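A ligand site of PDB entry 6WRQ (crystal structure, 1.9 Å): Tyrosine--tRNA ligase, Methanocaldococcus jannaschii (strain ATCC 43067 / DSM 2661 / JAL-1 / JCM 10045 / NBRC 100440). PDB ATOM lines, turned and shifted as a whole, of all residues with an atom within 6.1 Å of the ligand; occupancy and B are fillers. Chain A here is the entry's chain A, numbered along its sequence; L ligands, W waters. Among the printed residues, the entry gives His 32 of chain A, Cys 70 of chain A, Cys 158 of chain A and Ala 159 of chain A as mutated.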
ATOM      1  N   HIS A  32       0.641  -0.240  21.834  1.00  0.00           N
ATOM      2  CA  HIS A  32      -0.644   0.353  21.500  1.00  0.00           C
ATOM      3  C   HIS A  32      -1.340  -0.299  20.332  1.00  0.00           C
ATOM      4  O   HIS A  32      -0.754  -0.999  19.583  1.00  0.00           O
ATOM      5  CB  HIS A  32      -0.624   1.880  21.364  1.00  0.00           C
ATOM      6  CG  HIS A  32      -0.240   2.409  20.016  1.00  0.00           C
ATOM      7  ND1 HIS A  32       0.086   3.726  19.829  1.00  0.00           N
ATOM      8  CD2 HIS A  32      -0.202   1.841  18.792  1.00  0.00           C
ATOM      9  CE1 HIS A  32       0.354   3.944  18.551  1.00  0.00           C
ATOM     10  NE2 HIS A  32       0.191   2.809  17.907  1.00  0.00           N
ATOM     11  N   ILE A  33      -2.620  -0.052  20.240  1.00  0.00           N
ATOM     12  CA  ILE A  33      -3.446  -0.531  19.149  1.00  0.00           C
ATOM     13  C   ILE A  33      -4.519   0.507  18.932  1.00  0.00           C
ATOM     14  O   ILE A  33      -5.050   1.088  19.888  1.00  0.00           O
ATOM     15  CB  ILE A  33      -4.003  -1.938  19.459  1.00  0.00           C
ATOM     16  CG1 ILE A  33      -4.922  -2.417  18.347  1.00  0.00           C
ATOM     17  CG2 ILE A  33      -4.775  -1.959  20.755  1.00  0.00           C
ATOM     18  CD1 ILE A  33      -5.166  -3.881  18.356  1.00  0.00           C
ATOM     19  N   GLY A  34      -4.890   0.729  17.680  1.00  0.00           N
ATOM     20  CA  GLY A  34      -5.961   1.638  17.354  1.00  0.00           C
ATOM     21  C   GLY A  34      -7.152   0.874  16.772  1.00  0.00           C
ATOM     22  O   GLY A  34      -6.956  -0.099  16.062  1.00  0.00           O
ATOM     23  N   PHE A  35      -8.339   1.329  17.124  1.00  0.00           N
ATOM     24  CA  PHE A  35      -9.562   0.788  16.537  1.00  0.00           C
ATOM     25  C   PHE A  35     -10.422   1.933  15.991  1.00  0.00           C
ATOM     26  O   PHE A  35     -10.817   2.820  16.741  1.00  0.00           O
ATOM     27  CB  PHE A  35     -10.420   0.024  17.570  1.00  0.00           C
ATOM     28  CG  PHE A  35      -9.775  -1.182  18.168  1.00  0.00           C
ATOM     29  CD1 PHE A  35      -9.719  -2.349  17.459  1.00  0.00           C
ATOM     30  CD2 PHE A  35      -9.302  -1.162  19.456  1.00  0.00           C
ATOM     31  CE1 PHE A  35      -9.157  -3.452  17.991  1.00  0.00           C
ATOM     32  CE2 PHE A  35      -8.751  -2.262  20.021  1.00  0.00           C
ATOM     33  CZ  PHE A  35      -8.671  -3.418  19.295  1.00  0.00           C
ATOM     34  N   GLU A  36     -10.778   1.867  14.719  1.00  0.00           N
ATOM     35  CA  GLU A  36     -11.911   2.652  14.266  1.00  0.00           C
ATOM     36  C   GLU A  36     -13.106   2.225  15.104  1.00  0.00           C
ATOM     37  O   GLU A  36     -13.390   1.031  15.163  1.00  0.00           O
ATOM     38  CB  GLU A  36     -12.199   2.410  12.803  1.00  0.00           C
ATOM     39  CG  GLU A  36     -11.099   2.917  11.872  1.00  0.00           C
ATOM     40  CD  GLU A  36     -11.504   2.858  10.428  1.00  0.00           C
ATOM     41  OE1 GLU A  36     -12.686   3.068  10.135  1.00  0.00           O
ATOM     42  OE2 GLU A  36     -10.649   2.603   9.562  1.00  0.00           O
ATOM     43  N   LEU A  65      -6.045   3.277  21.332  1.00  0.00           N
ATOM     44  CA  LEU A  65      -6.370   4.460  20.539  1.00  0.00           C
ATOM     45  C   LEU A  65      -7.770   4.263  19.950  1.00  0.00           C
ATOM     46  O   LEU A  65      -7.994   3.371  19.128  1.00  0.00           O
ATOM     47  CB  LEU A  65      -5.328   4.684  19.444  1.00  0.00           C
ATOM     48  CG  LEU A  65      -5.523   5.951  18.597  1.00  0.00           C
ATOM     49  CD1 LEU A  65      -5.050   7.159  19.476  1.00  0.00           C
ATOM     50  CD2 LEU A  65      -4.842   5.926  17.242  1.00  0.00           C
ATOM     51  N   ALA A  67      -9.835   5.502  17.379  1.00  0.00           N
ATOM     52  CA  ALA A  67      -9.291   6.156  16.187  1.00  0.00           C
ATOM     53  C   ALA A  67     -10.402   6.941  15.476  1.00  0.00           C
ATOM     54  O   ALA A  67     -10.861   6.606  14.374  1.00  0.00           O
ATOM     55  CB  ALA A  67      -8.663   5.120  15.253  1.00  0.00           C
ATOM     56  N   ASP A  68     -10.831   8.019  16.151  1.00  0.00           N
ATOM     57  CA  ASP A  68     -12.003   8.741  15.665  1.00  0.00           C
ATOM     58  C   ASP A  68     -11.678   9.465  14.367  1.00  0.00           C
ATOM     59  O   ASP A  68     -12.468   9.462  13.406  1.00  0.00           O
ATOM     60  CB  ASP A  68     -12.531   9.700  16.748  1.00  0.00           C
ATOM     61  CG  ASP A  68     -11.483  10.668  17.294  1.00  0.00           C
ATOM     62  OD1 ASP A  68     -10.246  10.481  17.185  1.00  0.00           O
ATOM     63  OD2 ASP A  68     -11.924  11.656  17.894  1.00  0.00           O
ATOM     64  N   LEU A  69     -10.531  10.083  14.350  1.00  0.00           N
ATOM     65  CA  LEU A  69     -10.136  10.888  13.174  1.00  0.00           C
ATOM     66  C   LEU A  69      -9.925   9.932  11.931  1.00  0.00           C
ATOM     67  O   LEU A  69     -10.399  10.190  10.848  1.00  0.00           O
ATOM     68  CB  LEU A  69      -8.887  11.779  13.412  1.00  0.00           C
ATOM     69  CG  LEU A  69      -8.579  12.797  12.318  1.00  0.00           C
ATOM     70  CD1 LEU A  69      -9.760  13.722  12.079  1.00  0.00           C
ATOM     71  CD2 LEU A  69      -7.295  13.574  12.606  1.00  0.00           C
ATOM     72  N   CYS A  70      -9.175   8.835  12.092  1.00  0.00           N
ATOM     73  CA  CYS A  70      -8.996   7.861  10.957  1.00  0.00           C
ATOM     74  C   CYS A  70     -10.425   7.315  10.536  1.00  0.00           C
ATOM     75  O   CYS A  70     -10.690   7.121   9.373  1.00  0.00           O
ATOM     76  CB  CYS A  70      -8.001   6.683  11.204  1.00  0.00           C
ATOM     77  SG  CYS A  70      -6.289   7.167  11.030  1.00  0.00           S
ATOM     78  N   GLY A 105      -7.871   9.701  19.005  1.00  0.00           N
ATOM     79  CA  GLY A 105      -6.877  10.198  18.086  1.00  0.00           C
ATOM     80  C   GLY A 105      -6.917  11.702  17.969  1.00  0.00           C
ATOM     81  O   GLY A 105      -5.870  12.355  17.899  1.00  0.00           O
ATOM     82  N   GLN A 109      -4.013  14.391  17.114  1.00  0.00           N
ATOM     83  CA  GLN A 109      -3.800  14.295  15.658  1.00  0.00           C
ATOM     84  C   GLN A 109      -4.076  15.572  14.842  1.00  0.00           C
ATOM     85  O   GLN A 109      -3.922  15.579  13.644  1.00  0.00           O
ATOM     86  CB  GLN A 109      -4.511  13.069  15.015  1.00  0.00           C
ATOM     87  CG  GLN A 109      -4.051  11.735  15.571  1.00  0.00           C
ATOM     88  CD  GLN A 109      -4.868  10.553  15.015  1.00  0.00           C
ATOM     89  OE1 GLN A 109      -6.056  10.671  14.921  1.00  0.00           O
ATOM     90  NE2 GLN A 109      -4.245   9.453  14.679  1.00  0.00           N
ATOM     91  N   TYR A 114       1.926  17.533  14.800  1.00  0.00           N
ATOM     92  CA  TYR A 114       1.471  16.303  14.140  1.00  0.00           C
ATOM     93  C   TYR A 114       1.233  16.545  12.638  1.00  0.00           C
ATOM     94  O   TYR A 114       1.724  15.797  11.772  1.00  0.00           O
ATOM     95  CB  TYR A 114       0.173  15.809  14.806  1.00  0.00           C
ATOM     96  CG  TYR A 114      -0.147  14.357  14.589  1.00  0.00           C
ATOM     97  CD1 TYR A 114      -0.689  13.922  13.387  1.00  0.00           C
ATOM     98  CD2 TYR A 114       0.121  13.412  15.565  1.00  0.00           C
ATOM     99  CE1 TYR A 114      -1.002  12.546  13.152  1.00  0.00           C
ATOM    100  CE2 TYR A 114      -0.148  12.085  15.372  1.00  0.00           C
ATOM    101  CZ  TYR A 114      -0.702  11.644  14.166  1.00  0.00           C
ATOM    102  OH  TYR A 114      -0.956  10.297  14.012  1.00  0.00           O
ATOM    103  N   ILE A 137      -8.391  -2.129   4.271  1.00  0.00           N
ATOM    104  CA  ILE A 137      -8.896  -1.253   5.316  1.00  0.00           C
ATOM    105  C   ILE A 137      -9.921  -0.257   4.775  1.00  0.00           C
ATOM    106  O   ILE A 137     -10.906   0.061   5.450  1.00  0.00           O
ATOM    107  CB  ILE A 137      -7.719  -0.495   5.981  1.00  0.00           C
ATOM    108  CG1 ILE A 137      -6.811  -1.466   6.724  1.00  0.00           C
ATOM    109  CG2 ILE A 137      -8.258   0.617   6.902  1.00  0.00           C
ATOM    110  CD1 ILE A 137      -5.473  -0.854   7.061  1.00  0.00           C
ATOM    111  N   TYR A 151      -5.209   8.697   5.371  1.00  0.00           N
ATOM    112  CA  TYR A 151      -5.343   7.749   6.478  1.00  0.00           C
ATOM    113  C   TYR A 151      -4.053   7.014   6.823  1.00  0.00           C
ATOM    114  O   TYR A 151      -3.665   7.033   7.988  1.00  0.00           O
ATOM    115  CB  TYR A 151      -6.452   6.781   6.132  1.00  0.00           C
ATOM    116  CG  TYR A 151      -6.849   5.738   7.154  1.00  0.00           C
ATOM    117  CD1 TYR A 151      -6.008   4.723   7.494  1.00  0.00           C
ATOM    118  CD2 TYR A 151      -8.140   5.721   7.641  1.00  0.00           C
ATOM    119  CE1 TYR A 151      -6.424   3.700   8.382  1.00  0.00           C
ATOM    120  CE2 TYR A 151      -8.588   4.714   8.504  1.00  0.00           C
ATOM    121  CZ  TYR A 151      -7.698   3.742   8.907  1.00  0.00           C
ATOM    122  OH  TYR A 151      -8.091   2.707   9.744  1.00  0.00           O
ATOM    123  N   MET A 154      -1.533   9.209   8.530  1.00  0.00           N
ATOM    124  CA  MET A 154      -1.997   9.512   9.867  1.00  0.00           C
ATOM    125  C   MET A 154      -1.574   8.417  10.835  1.00  0.00           C
ATOM    126  O   MET A 154      -1.051   8.689  11.917  1.00  0.00           O
ATOM    127  CB  MET A 154      -3.525   9.667   9.849  1.00  0.00           C
ATOM    128  CG  MET A 154      -4.158  10.019  11.168  1.00  0.00           C
ATOM    129  SD  MET A 154      -3.660  11.639  11.759  1.00  0.00           S
ATOM    130  CE  MET A 154      -4.434  12.723  10.584  1.00  0.00           C
ATOM    131  N   GLN A 155      -1.803   7.165  10.444  1.00  0.00           N
ATOM    132  CA  GLN A 155      -1.487   6.030  11.316  1.00  0.00           C
ATOM    133  C   GLN A 155       0.022   5.890  11.505  1.00  0.00           C
ATOM    134  O   GLN A 155       0.500   5.677  12.634  1.00  0.00           O
ATOM    135  CB  GLN A 155      -2.111   4.752  10.748  1.00  0.00           C
ATOM    136  CG  GLN A 155      -1.901   3.527  11.608  1.00  0.00           C
ATOM    137  CD  GLN A 155      -2.843   2.412  11.234  1.00  0.00           C
ATOM    138  OE1 GLN A 155      -3.918   2.667  10.709  1.00  0.00           O
ATOM    139  NE2 GLN A 155      -2.432   1.182  11.483  1.00  0.00           N
ATOM    140  N   VAL A 156       0.757   6.066  10.439  1.00  0.00           N
ATOM    141  CA  VAL A 156       2.213   5.957  10.507  1.00  0.00           C
ATOM    142  C   VAL A 156       2.713   7.038  11.538  1.00  0.00           C
ATOM    143  O   VAL A 156       3.426   6.769  12.482  1.00  0.00           O
ATOM    144  CB  VAL A 156       2.963   6.239   9.163  1.00  0.00           C
ATOM    145  CG1 VAL A 156       4.446   6.454   9.404  1.00  0.00           C
ATOM    146  CG2 VAL A 156       2.668   5.167   8.125  1.00  0.00           C
ATOM    147  N   CYS A 158       1.122   8.471  13.981  1.00  0.00           N
ATOM    148  CA  CYS A 158       0.642   8.099  15.321  1.00  0.00           C
ATOM    149  C   CYS A 158       1.749   7.277  16.108  1.00  0.00           C
ATOM    150  O   CYS A 158       2.065   7.585  17.235  1.00  0.00           O
ATOM    151  CB  CYS A 158      -0.666   7.241  15.354  1.00  0.00           C
ATOM    152  SG  CYS A 158      -1.347   7.063  16.965  1.00  0.00           S
ATOM    153  N   ALA A 159       2.319   6.241  15.493  1.00  0.00           N
ATOM    154  CA  ALA A 159       3.355   5.455  16.207  1.00  0.00           C
ATOM    155  C   ALA A 159       4.541   6.384  16.586  1.00  0.00           C
ATOM    156  O   ALA A 159       5.124   6.290  17.630  1.00  0.00           O
ATOM    157  CB  ALA A 159       3.918   4.244  15.429  1.00  0.00           C
ATOM    158  N   GLU A 172      -4.330  -7.053   8.472  1.00  0.00           N
ATOM    159  CA  GLU A 172      -4.720  -6.047   7.495  1.00  0.00           C
ATOM    160  C   GLU A 172      -3.871  -4.785   7.628  1.00  0.00           C
ATOM    161  O   GLU A 172      -3.767  -4.016   6.677  1.00  0.00           O
ATOM    162  CB  GLU A 172      -6.220  -5.679   7.613  1.00  0.00           C
ATOM    163  CG  GLU A 172      -6.607  -4.817   8.807  1.00  0.00           C
ATOM    164  CD  GLU A 172      -6.695  -5.605  10.112  1.00  0.00           C
ATOM    165  OE1 GLU A 172      -6.958  -4.993  11.162  1.00  0.00           O
ATOM    166  OE2 GLU A 172      -6.460  -6.847  10.069  1.00  0.00           O
ATOM    167  N   GLN A 173      -3.295  -4.555   8.796  1.00  0.00           N
ATOM    168  CA  GLN A 173      -2.534  -3.354   9.052  1.00  0.00           C
ATOM    169  C   GLN A 173      -1.095  -3.483   8.621  1.00  0.00           C
ATOM    170  O   GLN A 173      -0.360  -2.522   8.776  1.00  0.00           O
ATOM    171  CB  GLN A 173      -2.541  -3.032  10.560  1.00  0.00           C
ATOM    172  CG  GLN A 173      -3.905  -3.115  11.207  1.00  0.00           C
ATOM    173  CD  GLN A 173      -4.829  -2.006  10.790  1.00  0.00           C
ATOM    174  OE1 GLN A 173      -4.421  -0.863  10.682  1.00  0.00           O
ATOM    175  NE2 GLN A 173      -6.085  -2.341  10.552  1.00  0.00           N
ATOM    176  N   ILE A 176       0.691  -0.744   6.230  1.00  0.00           N
ATOM    177  CA  ILE A 176       0.878   0.532   6.904  1.00  0.00           C
ATOM    178  C   ILE A 176       2.036   0.440   7.905  1.00  0.00           C
ATOM    179  O   ILE A 176       2.848   1.357   8.043  1.00  0.00           O
ATOM    180  CB  ILE A 176      -0.438   0.982   7.600  1.00  0.00           C
ATOM    181  CG1 ILE A 176      -1.499   1.363   6.579  1.00  0.00           C
ATOM    182  CG2 ILE A 176      -0.124   2.067   8.637  1.00  0.00           C
ATOM    183  CD1 ILE A 176      -2.881   1.579   7.213  1.00  0.00           C
ATOM    184  N   HIS A 177       2.085  -0.656   8.669  1.00  0.00           N
ATOM    185  CA  HIS A 177       3.184  -0.832   9.626  1.00  0.00           C
ATOM    186  C   HIS A 177       4.540  -0.964   8.937  1.00  0.00           C
ATOM    187  O   HIS A 177       5.550  -0.417   9.427  1.00  0.00           O
ATOM    188  CB  HIS A 177       2.887  -2.023  10.495  1.00  0.00           C
ATOM    189  CG  HIS A 177       1.820  -1.774  11.494  1.00  0.00           C
ATOM    190  ND1 HIS A 177       1.199  -2.800  12.172  1.00  0.00           N
ATOM    191  CD2 HIS A 177       1.280  -0.624  11.954  1.00  0.00           C
ATOM    192  CE1 HIS A 177       0.351  -2.275  13.043  1.00  0.00           C
ATOM    193  NE2 HIS A 177       0.369  -0.961  12.923  1.00  0.00           N
HETATM  194  N1  LIG L   1      -6.296   1.191  10.985  1.00  0.00           N
HETATM  195  C1  LIG L   1      -6.960   0.751  12.235  1.00  0.00           C
HETATM  196  C2  LIG L   1      -8.251   0.024  11.939  1.00  0.00           C
HETATM  197  O1  LIG L   1      -8.395  -0.484  10.828  1.00  0.00           O
HETATM  198  C3  LIG L   1      -7.208   1.943  13.148  1.00  0.00           C
HETATM  199  C4  LIG L   1      -5.949   2.674  13.648  1.00  0.00           C
HETATM  200  C5  LIG L   1      -5.863   4.059  13.614  1.00  0.00           C
HETATM  201  C6  LIG L   1      -4.905   1.963  14.210  1.00  0.00           C
HETATM  202  C7  LIG L   1      -4.737   4.729  14.084  1.00  0.00           C
HETATM  203  C8  LIG L   1      -3.781   2.604  14.682  1.00  0.00           C
HETATM  204  C9  LIG L   1      -3.688   3.994  14.619  1.00  0.00           C
HETATM  205  O2  LIG L   1      -2.587   4.637  15.082  1.00  0.00           O
HETATM  206  N2  LIG L   1      -4.682   6.135  14.011  1.00  0.00           N
HETATM  207  O3  LIG L   1      -5.682   6.744  14.063  1.00  0.00           O
HETATM  208  O4  LIG L   1      -3.675   6.723  13.884  1.00  0.00           O
HETATM  209  O5  LIG L   1      -9.142  -0.052  12.807  1.00  0.00           O
HETATM  210  O   HOH W   1       0.098   3.367  15.041  1.00  0.00           O
HETATM  211  O   HOH W   2     -10.812  -1.575   9.660  1.00  0.00           O
HETATM  212  O   HOH W   3      -7.641   8.645  14.704  1.00  0.00           O
HETATM  213  O   HOH W   4      -3.059  -0.670  15.631  1.00  0.00           O
HETATM  214  O   HOH W   5     -10.382  -2.128  13.531  1.00  0.00           O
HETATM  215  O   HOH W   6      -5.301  -1.533  14.292  1.00  0.00           O
HETATM  216  O   HOH W   7      -0.950   0.768  14.581  1.00  0.00           O
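An oxygen (O3) of the ligand sits at hydrogen-bond distance from the side-chain sulfur (SG) of Cys 70 (3.1 Å).
The side-chain sulfur (SG) of Cys 158 lies close to an oxygen (O2) of the ligand.
OE1 of Gln 173 sits at hydrogen-bond distance from N1 of the ligand, 2.8 Å away.
OH of Tyr 151 sits at hydrogen-bond distance from N1 of the ligand.
A nitrogen (N1) of the ligand sits at hydrogen-bond distance from the side-chain amide oxygen (OE1) of Gln 155 (2.8 Å).
The side-chain amide nitrogen of Gln 109 sits at hydrogen-bond distance from an oxygen (O4) of the ligand (2.9 Å).
An oxygen (O5) of the ligand lies within hydrogen-bond range of the backbone NH (N) of Glu 36.
The backbone NH of Cys 158 lies within hydrogen-bond range of the side-chain hydroxyl of Tyr 114 (2.8 Å).
The side-chain hydroxyl (OH) of Tyr 114 is in hydrogen-bond range of the backbone carbonyl oxygen (O) of Met 154, 2.6 Å away.
The side-chain hydroxyl (OH) of Tyr 114 sits at hydrogen-bond distance from the side-chain amide nitrogen (NE2) of Gln 109 (3.5 Å).
The side-chain sulfur (SD) of Met 154 lies close to the side-chain amide nitrogen (NE2) of Gln 109 (3.7 Å).
The side-chain hydroxyl (OH) of Tyr 151 is in hydrogen-bond range of the side-chain carboxylate (OE2) of Glu 36 (2.6 Å).
The side-chain amide nitrogen (NE2) of Gln 173 lies within hydrogen-bond range of the side-chain carboxylate (OE1) of Glu 172, at 2.9 Å.
N of Leu 65 is in hydrogen-bond range of O of Ile 33 (2.8 Å).
The backbone carbonyl oxygen (O) of Leu 65 lies within hydrogen-bond range of the backbone NH (N) of Phe 35.
Merely in contact with the ligand: Leu 65 (3.2 Å), Gly 34 (3.3 Å), Ala 67 (3.4 Å), Met 154 (3.8 Å) and Phe 35 (3.8 Å).
Hydrophobic or aromatic side chains within 4 Å of the ligand: Leu 65, Ala 67 and Tyr 151.
Of the 24 residues printed, 12 come within 4 Å of the ligand.
The nearest printed residue that does not touch the ligand is Ile 137 (4.1 Å).
Water W3 lies within hydrogen-bond range of OE1 of Gln 109 (2.6 Å), O3 of the ligand (2.8 Å), N of Cys 70 (3.0 Å) and N of Leu 69 (3.2 Å).
Water W1 lies within hydrogen-bond range of a ring nitrogen (NE2) of His 32 (2.9 Å), an oxygen (O2) of the ligand (3.0 Å) and the backbone carbonyl oxygen (O) of Gln 155 (3.4 Å).
Water W7 bridges a ring nitrogen (NE2) of His 177 and the side-chain amide nitrogen (NE2) of Gln 155.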
